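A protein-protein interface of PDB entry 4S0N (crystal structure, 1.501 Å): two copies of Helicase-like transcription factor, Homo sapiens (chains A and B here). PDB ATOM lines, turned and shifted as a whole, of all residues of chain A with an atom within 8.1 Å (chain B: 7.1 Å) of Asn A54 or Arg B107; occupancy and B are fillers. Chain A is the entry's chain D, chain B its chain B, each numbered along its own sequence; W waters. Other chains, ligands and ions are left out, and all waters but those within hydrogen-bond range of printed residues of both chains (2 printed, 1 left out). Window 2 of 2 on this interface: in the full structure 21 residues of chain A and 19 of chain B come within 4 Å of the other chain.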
ATOM      1  N   VAL A  26     -16.229  -1.456  -7.381  1.00  0.00           N
ATOM      2  CA  VAL A  26     -17.030  -0.751  -6.391  1.00  0.00           C
ATOM      3  C   VAL A  26     -16.610  -1.147  -4.981  1.00  0.00           C
ATOM      4  O   VAL A  26     -16.381  -2.321  -4.706  1.00  0.00           O
ATOM      5  CB  VAL A  26     -18.525  -1.036  -6.595  1.00  0.00           C
ATOM      6  CG1 VAL A  26     -19.359  -0.394  -5.492  1.00  0.00           C
ATOM      7  CG2 VAL A  26     -18.970  -0.529  -7.973  1.00  0.00           C
ATOM      8  N   GLU A  31     -15.744  -1.462   4.289  1.00  0.00           N
ATOM      9  CA  GLU A  31     -15.251  -2.673   3.637  1.00  0.00           C
ATOM     10  C   GLU A  31     -13.723  -2.748   3.627  1.00  0.00           C
ATOM     11  O   GLU A  31     -13.033  -1.735   3.454  1.00  0.00           O
ATOM     12  CB  GLU A  31     -15.750  -2.777   2.192  1.00  0.00           C
ATOM     13  CG  GLU A  31     -17.256  -2.976   2.088  1.00  0.00           C
ATOM     14  CD  GLU A  31     -17.728  -3.266   0.672  1.00  0.00           C
ATOM     15  OE1 GLU A  31     -16.904  -3.181  -0.278  1.00  0.00           O
ATOM     16  OE2 GLU A  31     -18.935  -3.596   0.521  1.00  0.00           O
ATOM     17  N   MET A  32     -13.215  -3.962   3.811  1.00  0.00           N
ATOM     18  CA  MET A  32     -11.844  -4.294   3.441  1.00  0.00           C
ATOM     19  C   MET A  32     -11.579  -3.995   1.992  1.00  0.00           C
ATOM     20  O   MET A  32     -12.454  -4.184   1.144  1.00  0.00           O
ATOM     21  CB  MET A  32     -11.567  -5.785   3.616  1.00  0.00           C
ATOM     22  CG  MET A  32     -11.274  -6.229   4.977  1.00  0.00           C
ATOM     23  SD  MET A  32     -10.611  -7.898   4.917  1.00  0.00           S
ATOM     24  CE  MET A  32     -11.997  -8.771   4.200  1.00  0.00           C
ATOM     25  N   VAL A  33     -10.347  -3.607   1.703  1.00  0.00           N
ATOM     26  CA  VAL A  33      -9.859  -3.616   0.339  1.00  0.00           C
ATOM     27  C   VAL A  33      -8.547  -4.379   0.332  1.00  0.00           C
ATOM     28  O   VAL A  33      -7.899  -4.525   1.376  1.00  0.00           O
ATOM     29  CB  VAL A  33      -9.670  -2.194  -0.228  1.00  0.00           C
ATOM     30  CG1 VAL A  33     -11.029  -1.509  -0.420  1.00  0.00           C
ATOM     31  CG2 VAL A  33      -8.753  -1.378   0.667  1.00  0.00           C
ATOM     32  N   ALA A  34      -8.155  -4.873  -0.837  1.00  0.00           N
ATOM     33  CA  ALA A  34      -6.895  -5.583  -0.965  1.00  0.00           C
ATOM     34  C   ALA A  34      -5.814  -4.644  -1.474  1.00  0.00           C
ATOM     35  O   ALA A  34      -6.042  -3.894  -2.426  1.00  0.00           O
ATOM     36  CB  ALA A  34      -7.046  -6.757  -1.902  1.00  0.00           C
ATOM     37  N   ASN A  51      -7.850  -3.212  -4.679  1.00  0.00           N
ATOM     38  CA  ASN A  51      -8.971  -3.968  -5.217  1.00  0.00           C
ATOM     39  C   ASN A  51     -10.039  -4.132  -4.168  1.00  0.00           C
ATOM     40  O   ASN A  51      -9.731  -4.116  -2.978  1.00  0.00           O
ATOM     41  CB  ASN A  51      -8.527  -5.362  -5.684  1.00  0.00           C
ATOM     42  CG  ASN A  51      -7.328  -5.319  -6.626  1.00  0.00           C
ATOM     43  OD1 ASN A  51      -7.240  -4.465  -7.516  1.00  0.00           O
ATOM     44  ND2 ASN A  51      -6.401  -6.251  -6.434  1.00  0.00           N
ATOM     45  N   ASN A  52     -11.288  -4.321  -4.587  1.00  0.00           N
ATOM     46  CA  ASN A  52     -12.309  -4.683  -3.616  1.00  0.00           C
ATOM     47  C   ASN A  52     -12.153  -6.161  -3.247  1.00  0.00           C
ATOM     48  O   ASN A  52     -11.278  -6.862  -3.782  1.00  0.00           O
ATOM     49  CB  ASN A  52     -13.730  -4.358  -4.123  1.00  0.00           C
ATOM     50  CG  ASN A  52     -14.146  -5.165  -5.348  1.00  0.00           C
ATOM     51  OD1 ASN A  52     -13.585  -6.212  -5.648  1.00  0.00           O
ATOM     52  ND2 ASN A  52     -15.171  -4.677  -6.044  1.00  0.00           N
ATOM     53  N   VAL A  53     -12.976  -6.644  -2.328  1.00  0.00           N
ATOM     54  CA  VAL A  53     -12.774  -8.015  -1.846  1.00  0.00           C
ATOM     55  C   VAL A  53     -13.093  -9.045  -2.924  1.00  0.00           C
ATOM     56  O   VAL A  53     -12.571 -10.157  -2.869  1.00  0.00           O
ATOM     57  CB  VAL A  53     -13.592  -8.342  -0.579  1.00  0.00           C
ATOM     58  CG1 VAL A  53     -13.033  -7.572   0.611  1.00  0.00           C
ATOM     59  CG2 VAL A  53     -15.085  -8.093  -0.793  1.00  0.00           C
ATOM     60  N   ASN A  54     -13.898  -8.674  -3.926  1.00  0.00           N
ATOM     61  CA  ASN A  54     -14.167  -9.569  -5.060  1.00  0.00           C
ATOM     62  C   ASN A  54     -13.033  -9.615  -6.093  1.00  0.00           C
ATOM     63  O   ASN A  54     -13.060 -10.423  -7.033  1.00  0.00           O
ATOM     64  CB  ASN A  54     -15.467  -9.169  -5.753  1.00  0.00           C
ATOM     65  CG  ASN A  54     -16.704  -9.517  -4.921  1.00  0.00           C
ATOM     66  OD1 ASN A  54     -16.673 -10.427  -4.088  1.00  0.00           O
ATOM     67  ND2 ASN A  54     -17.793  -8.792  -5.146  1.00  0.00           N
ATOM     68  N   GLY A  55     -12.040  -8.751  -5.907  1.00  0.00           N
ATOM     69  CA  GLY A  55     -10.861  -8.723  -6.753  1.00  0.00           C
ATOM     70  C   GLY A  55     -10.886  -7.698  -7.871  1.00  0.00           C
ATOM     71  O   GLY A  55      -9.935  -7.620  -8.650  1.00  0.00           O
ATOM     72  N   ASN A  56     -11.960  -6.913  -7.956  1.00  0.00           N
ATOM     73  CA  ASN A  56     -12.057  -5.849  -8.959  1.00  0.00           C
ATOM     74  C   ASN A  56     -11.224  -4.638  -8.563  1.00  0.00           C
ATOM     75  O   ASN A  56     -11.339  -4.161  -7.437  1.00  0.00           O
ATOM     76  CB  ASN A  56     -13.509  -5.397  -9.157  1.00  0.00           C
ATOM     77  CG  ASN A  56     -14.475  -6.550  -9.306  1.00  0.00           C
ATOM     78  OD1 ASN A  56     -15.463  -6.644  -8.572  1.00  0.00           O
ATOM     79  ND2 ASN A  56     -14.203  -7.429 -10.258  1.00  0.00           N
ATOM     80  N   GLN A  57     -10.409  -4.115  -9.476  1.00  0.00           N
ATOM     81  CA  GLN A  57      -9.597  -2.948  -9.121  1.00  0.00           C
ATOM     82  C   GLN A  57     -10.456  -1.698  -8.891  1.00  0.00           C
ATOM     83  O   GLN A  57     -11.361  -1.386  -9.671  1.00  0.00           O
ATOM     84  CB  GLN A  57      -8.531  -2.649 -10.186  1.00  0.00           C
ATOM     85  CG  GLN A  57      -7.558  -1.580  -9.705  1.00  0.00           C
ATOM     86  CD  GLN A  57      -6.343  -1.415 -10.589  1.00  0.00           C
ATOM     87  OE1 GLN A  57      -6.197  -2.097 -11.602  1.00  0.00           O
ATOM     88  NE2 GLN A  57      -5.455  -0.508 -10.199  1.00  0.00           N
ATOM     89  N   VAL B   8      -4.360 -13.829  -3.417  1.00  0.00           N
ATOM     90  CA  VAL B   8      -5.179 -12.624  -3.331  1.00  0.00           C
ATOM     91  C   VAL B   8      -6.280 -12.782  -2.276  1.00  0.00           C
ATOM     92  O   VAL B   8      -6.661 -13.896  -1.883  1.00  0.00           O
ATOM     93  CB  VAL B   8      -5.836 -12.264  -4.690  1.00  0.00           C
ATOM     94  CG1 VAL B   8      -4.776 -12.035  -5.761  1.00  0.00           C
ATOM     95  CG2 VAL B   8      -6.824 -13.336  -5.119  1.00  0.00           C
ATOM     96  N   LEU B   9      -6.799 -11.653  -1.824  1.00  0.00           N
ATOM     97  CA  LEU B   9      -7.855 -11.632  -0.821  1.00  0.00           C
ATOM     98  C   LEU B   9      -9.203 -12.096  -1.373  1.00  0.00           C
ATOM     99  O   LEU B   9      -9.660 -11.589  -2.400  1.00  0.00           O
ATOM    100  CB  LEU B   9      -7.978 -10.212  -0.267  1.00  0.00           C
ATOM    101  CG  LEU B   9      -9.075  -9.957   0.764  1.00  0.00           C
ATOM    102  CD1 LEU B   9      -8.823 -10.766   2.044  1.00  0.00           C
ATOM    103  CD2 LEU B   9      -9.172  -8.465   1.074  1.00  0.00           C
ATOM    104  N   PHE B  10      -9.832 -13.058  -0.697  1.00  0.00           N
ATOM    105  CA  PHE B  10     -11.161 -13.544  -1.091  1.00  0.00           C
ATOM    106  C   PHE B  10     -12.275 -12.946  -0.231  1.00  0.00           C
ATOM    107  O   PHE B  10     -13.428 -12.871  -0.666  1.00  0.00           O
ATOM    108  CB  PHE B  10     -11.258 -15.073  -0.987  1.00  0.00           C
ATOM    109  CG  PHE B  10     -10.442 -15.831  -1.996  1.00  0.00           C
ATOM    110  CD1 PHE B  10      -9.950 -15.230  -3.147  1.00  0.00           C
ATOM    111  CD2 PHE B  10     -10.238 -17.191  -1.808  1.00  0.00           C
ATOM    112  CE1 PHE B  10      -9.218 -15.983  -4.077  1.00  0.00           C
ATOM    113  CE2 PHE B  10      -9.520 -17.938  -2.718  1.00  0.00           C
ATOM    114  CZ  PHE B  10      -9.014 -17.340  -3.859  1.00  0.00           C
ATOM    115  N   GLY B  11     -11.941 -12.542   0.995  1.00  0.00           N
ATOM    116  CA  GLY B  11     -12.941 -12.040   1.925  1.00  0.00           C
ATOM    117  C   GLY B  11     -12.848 -12.685   3.288  1.00  0.00           C
ATOM    118  O   GLY B  11     -11.912 -13.446   3.551  1.00  0.00           O
ATOM    119  N   LEU B  77      -7.511 -24.847  -1.424  1.00  0.00           N
ATOM    120  CA  LEU B  77      -8.187 -23.848  -2.246  1.00  0.00           C
ATOM    121  C   LEU B  77      -8.032 -22.450  -1.662  1.00  0.00           C
ATOM    122  O   LEU B  77      -8.131 -21.459  -2.384  1.00  0.00           O
ATOM    123  CB  LEU B  77      -9.664 -24.195  -2.403  1.00  0.00           C
ATOM    124  CG  LEU B  77      -9.948 -25.448  -3.230  1.00  0.00           C
ATOM    125  CD1 LEU B  77     -11.430 -25.772  -3.196  1.00  0.00           C
ATOM    126  CD2 LEU B  77      -9.468 -25.265  -4.660  1.00  0.00           C
ATOM    127  N   GLY B 102      -6.240 -16.752  -1.555  1.00  0.00           N
ATOM    128  CA  GLY B 102      -5.947 -17.830  -2.481  1.00  0.00           C
ATOM    129  C   GLY B 102      -5.612 -17.355  -3.878  1.00  0.00           C
ATOM    130  O   GLY B 102      -5.568 -16.161  -4.137  1.00  0.00           O
ATOM    131  N   LYS B 103      -5.377 -18.299  -4.779  1.00  0.00           N
ATOM    132  CA  LYS B 103      -5.130 -17.959  -6.169  1.00  0.00           C
ATOM    133  C   LYS B 103      -6.439 -17.570  -6.829  1.00  0.00           C
ATOM    134  O   LYS B 103      -7.486 -18.174  -6.555  1.00  0.00           O
ATOM    135  CB  LYS B 103      -4.487 -19.135  -6.901  1.00  0.00           C
ATOM    136  CG  LYS B 103      -3.212 -19.625  -6.237  1.00  0.00           C
ATOM    137  CD  LYS B 103      -2.727 -20.908  -6.881  1.00  0.00           C
ATOM    138  CE  LYS B 103      -1.739 -21.639  -5.983  1.00  0.00           C
ATOM    139  NZ  LYS B 103      -1.368 -22.959  -6.558  1.00  0.00           N
ATOM    140  N   GLU B 104      -6.379 -16.575  -7.708  1.00  0.00           N
ATOM    141  CA  GLU B 104      -7.584 -16.050  -8.337  1.00  0.00           C
ATOM    142  C   GLU B 104      -8.394 -17.167  -9.008  1.00  0.00           C
ATOM    143  O   GLU B 104      -9.622 -17.154  -8.967  1.00  0.00           O
ATOM    144  CB  GLU B 104      -7.218 -14.952  -9.341  1.00  0.00           C
ATOM    145  CG  GLU B 104      -8.395 -14.165  -9.889  1.00  0.00           C
ATOM    146  CD  GLU B 104      -9.283 -13.538  -8.810  1.00  0.00           C
ATOM    147  OE1 GLU B 104      -8.795 -12.756  -7.963  1.00  0.00           O
ATOM    148  OE2 GLU B 104     -10.492 -13.818  -8.830  1.00  0.00           O
ATOM    149  N   GLU B 105      -7.709 -18.157  -9.578  1.00  0.00           N
ATOM    150  CA  GLU B 105      -8.391 -19.256 -10.255  1.00  0.00           C
ATOM    151  C   GLU B 105      -9.217 -20.144  -9.329  1.00  0.00           C
ATOM    152  O   GLU B 105     -10.064 -20.909  -9.799  1.00  0.00           O
ATOM    153  CB  GLU B 105      -7.380 -20.130 -10.992  1.00  0.00           C
ATOM    154  CG  GLU B 105      -6.739 -19.470 -12.187  1.00  0.00           C
ATOM    155  CD  GLU B 105      -5.466 -18.716 -11.839  1.00  0.00           C
ATOM    156  OE1 GLU B 105      -5.171 -18.524 -10.633  1.00  0.00           O
ATOM    157  OE2 GLU B 105      -4.755 -18.321 -12.785  1.00  0.00           O
ATOM    158  N   ASN B 106      -8.963 -20.053  -8.024  1.00  0.00           N
ATOM    159  CA  ASN B 106      -9.698 -20.838  -7.036  1.00  0.00           C
ATOM    160  C   ASN B 106     -10.829 -20.074  -6.349  1.00  0.00           C
ATOM    161  O   ASN B 106     -11.545 -20.639  -5.507  1.00  0.00           O
ATOM    162  CB  ASN B 106      -8.721 -21.383  -5.983  1.00  0.00           C
ATOM    163  CG  ASN B 106      -7.922 -22.561  -6.509  1.00  0.00           C
ATOM    164  OD1 ASN B 106      -8.391 -23.281  -7.389  1.00  0.00           O
ATOM    165  ND2 ASN B 106      -6.712 -22.753  -5.995  1.00  0.00           N
ATOM    166  N   ARG B 107     -11.007 -18.807  -6.710  1.00  0.00           N
ATOM    167  CA  ARG B 107     -12.003 -17.976  -6.026  1.00  0.00           C
ATOM    168  C   ARG B 107     -13.413 -18.558  -6.157  1.00  0.00           C
ATOM    169  O   ARG B 107     -14.140 -18.662  -5.165  1.00  0.00           O
ATOM    170  CB  ARG B 107     -11.973 -16.534  -6.563  1.00  0.00           C
ATOM    171  CG  ARG B 107     -12.985 -15.631  -5.897  1.00  0.00           C
ATOM    172  CD  ARG B 107     -13.034 -14.265  -6.539  1.00  0.00           C
ATOM    173  NE  ARG B 107     -11.788 -13.511  -6.429  1.00  0.00           N
ATOM    174  CZ  ARG B 107     -11.490 -12.683  -5.429  1.00  0.00           C
ATOM    175  NH1 ARG B 107     -12.323 -12.549  -4.401  1.00  0.00           N
ATOM    176  NH2 ARG B 107     -10.341 -12.018  -5.445  1.00  0.00           N
ATOM    177  N   LYS B 108     -13.796 -18.976  -7.364  1.00  0.00           N
ATOM    178  CA  LYS B 108     -15.140 -19.514  -7.548  1.00  0.00           C
ATOM    179  C   LYS B 108     -15.329 -20.829  -6.787  1.00  0.00           C
ATOM    180  O   LYS B 108     -16.385 -21.068  -6.193  1.00  0.00           O
ATOM    181  CB  LYS B 108     -15.452 -19.728  -9.040  1.00  0.00           C
ATOM    182  CG  LYS B 108     -16.853 -20.296  -9.267  1.00  0.00           C
ATOM    183  CD  LYS B 108     -17.209 -20.460 -10.734  1.00  0.00           C
ATOM    184  CE  LYS B 108     -18.469 -21.311 -10.891  1.00  0.00           C
ATOM    185  NZ  LYS B 108     -19.603 -20.724 -10.141  1.00  0.00           N
ATOM    186  N   ALA B 109     -14.319 -21.693  -6.816  1.00  0.00           N
ATOM    187  CA  ALA B 109     -14.426 -22.971  -6.114  1.00  0.00           C
ATOM    188  C   ALA B 109     -14.650 -22.766  -4.604  1.00  0.00           C
ATOM    189  O   ALA B 109     -15.430 -23.483  -3.967  1.00  0.00           O
ATOM    190  CB  ALA B 109     -13.181 -23.813  -6.357  1.00  0.00           C
ATOM    191  N   VAL B 110     -13.960 -21.789  -4.038  1.00  0.00           N
ATOM    192  CA  VAL B 110     -14.119 -21.490  -2.620  1.00  0.00           C
ATOM    193  C   VAL B 110     -15.536 -21.000  -2.355  1.00  0.00           C
ATOM    194  O   VAL B 110     -16.207 -21.471  -1.437  1.00  0.00           O
ATOM    195  CB  VAL B 110     -13.085 -20.438  -2.152  1.00  0.00           C
ATOM    196  CG1 VAL B 110     -13.437 -19.883  -0.778  1.00  0.00           C
ATOM    197  CG2 VAL B 110     -11.688 -21.049  -2.132  1.00  0.00           C
ATOM    198  N   SER B 111     -16.006 -20.056  -3.158  1.00  0.00           N
ATOM    199  CA  SER B 111     -17.355 -19.538  -2.959  1.00  0.00           C
ATOM    200  C   SER B 111     -18.428 -20.600  -3.188  1.00  0.00           C
ATOM    201  O   SER B 111     -19.434 -20.636  -2.469  1.00  0.00           O
ATOM    202  CB  SER B 111     -17.602 -18.342  -3.867  1.00  0.00           C
ATOM    203  OG  SER B 111     -16.965 -17.201  -3.330  1.00  0.00           O
ATOM    204  N   ASP B 112     -18.219 -21.468  -4.176  1.00  0.00           N
ATOM    205  CA  ASP B 112     -19.166 -22.547  -4.420  1.00  0.00           C
ATOM    206  C   ASP B 112     -19.264 -23.482  -3.218  1.00  0.00           C
ATOM    207  O   ASP B 112     -20.356 -23.868  -2.812  1.00  0.00           O
ATOM    208  CB  ASP B 112     -18.774 -23.358  -5.659  1.00  0.00           C
ATOM    209  CG  ASP B 112     -18.989 -22.607  -6.962  1.00  0.00           C
ATOM    210  OD1 ASP B 112     -19.690 -21.576  -6.977  1.00  0.00           O
ATOM    211  OD2 ASP B 112     -18.451 -23.072  -7.991  1.00  0.00           O
ATOM    212  N   GLN B 113     -18.115 -23.848  -2.657  1.00  0.00           N
ATOM    213  CA  GLN B 113     -18.081 -24.777  -1.538  1.00  0.00           C
ATOM    214  C   GLN B 113     -18.750 -24.144  -0.323  1.00  0.00           C
ATOM    215  O   GLN B 113     -19.533 -24.793   0.380  1.00  0.00           O
ATOM    216  CB  GLN B 113     -16.644 -25.185  -1.209  1.00  0.00           C
ATOM    217  CG  GLN B 113     -16.495 -25.955   0.094  1.00  0.00           C
ATOM    218  CD  GLN B 113     -17.210 -27.302   0.115  1.00  0.00           C
ATOM    219  OE1 GLN B 113     -17.618 -27.836  -0.923  1.00  0.00           O
ATOM    220  NE2 GLN B 113     -17.363 -27.860   1.315  1.00  0.00           N
ATOM    221  N   LYS B 120     -21.178 -17.269   2.889  1.00  0.00           N
ATOM    222  CA  LYS B 120     -20.713 -16.363   1.854  1.00  0.00           C
ATOM    223  C   LYS B 120     -19.664 -15.415   2.424  1.00  0.00           C
ATOM    224  O   LYS B 120     -19.927 -14.716   3.407  1.00  0.00           O
ATOM    225  CB  LYS B 120     -21.879 -15.569   1.259  1.00  0.00           C
ATOM    226  CG  LYS B 120     -21.460 -14.652   0.126  1.00  0.00           C
ATOM    227  CD  LYS B 120     -22.640 -13.867  -0.436  1.00  0.00           C
ATOM    228  CE  LYS B 120     -22.205 -13.017  -1.610  1.00  0.00           C
ATOM    229  NZ  LYS B 120     -23.325 -12.170  -2.111  1.00  0.00           N
ATOM    230  N   LEU B 121     -18.471 -15.410   1.832  1.00  0.00           N
ATOM    231  CA  LEU B 121     -17.437 -14.459   2.234  1.00  0.00           C
ATOM    232  C   LEU B 121     -17.916 -13.017   2.078  1.00  0.00           C
ATOM    233  O   LEU B 121     -18.631 -12.674   1.126  1.00  0.00           O
ATOM    234  CB  LEU B 121     -16.165 -14.648   1.410  1.00  0.00           C
ATOM    235  CG  LEU B 121     -15.498 -16.013   1.599  1.00  0.00           C
ATOM    236  CD1 LEU B 121     -14.287 -16.117   0.687  1.00  0.00           C
ATOM    237  CD2 LEU B 121     -15.092 -16.244   3.066  1.00  0.00           C
HETATM  238  O   HOH W   1     -11.697 -11.314  -9.149  1.00  0.00           O
HETATM  239  O   HOH W   2     -15.901 -11.854  -1.551  1.00  0.00           O
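No position is printed for both chains.
Hydrophobic or aromatic side chains of chain A within 4 Å of the printed part of chain B: Ala A34 and Val A53. Among the printed residues, 6 pairs touch across the chains.
NE of Arg B107 lies close to O of Asn A54 (3.4 Å). The backbone carbonyl oxygen of Val A53 sits at hydrogen-bond distance from the guanidinium group of Arg B107 (2.9 Å). The backbone carbonyl oxygen (O) of Val A53 sits close to the backbone carbonyl oxygen (O) of Leu B9, at 3.3 Å.
Water W1 lies within hydrogen-bond range of the backbone carbonyl oxygen (O) of Asn A54 (2.7 Å), the side-chain carboxylate (OE2) of Glu B104 (2.8 Å) and the guanidinium group (NE) of Arg B107 (3.5 Å). Water W2 lies within hydrogen-bond range of O of Phe B10 (2.8 Å) and OD1 of Asn A54 (3.0 Å).
Asn A54 touches just one residue of chain B: Arg B107 (3.2 Å). Of the printed residues of chain A, Arg B107 touches Val A53, Asn A54 and Gly A55. Printed residues of chain A within 4 Å of Phe B10: Val A53. Of the printed residues of chain B, Gly A55 touches Arg B107. Of the printed residues of chain B, Ala A34 touches Leu B9 (3.9 Å). The nearest residue of chain B that does not touch Asn A54 is Glu B104 (4.6 Å).
N of Asn A54 sits at hydrogen-bond distance from OD1 of Asn A52, at 3.0 Å. The side-chain amide oxygen (OD1) of Asn A52 sits at hydrogen-bond distance from the backbone NH (N) of Gly A55 (3.0 Å). The backbone NH (N) of Ala A34 is in hydrogen-bond range of the backbone carbonyl oxygen (O) of Asn A51, 2.8 Å away. O of Leu B9 is in hydrogen-bond range of NH2 of Arg B107 (3.1 Å). OE2 of Glu B104 lies within salt-bridge range of NE of Arg B107, 2.7 Å away.
CB of Ala A34 touches CB of Leu B9, 3.9 Å away. O of Phe B10 touches O of Val A53, 3.6 Å away. Arg B107 touches Gly A55 (NH2 to CA, 3.6 Å).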
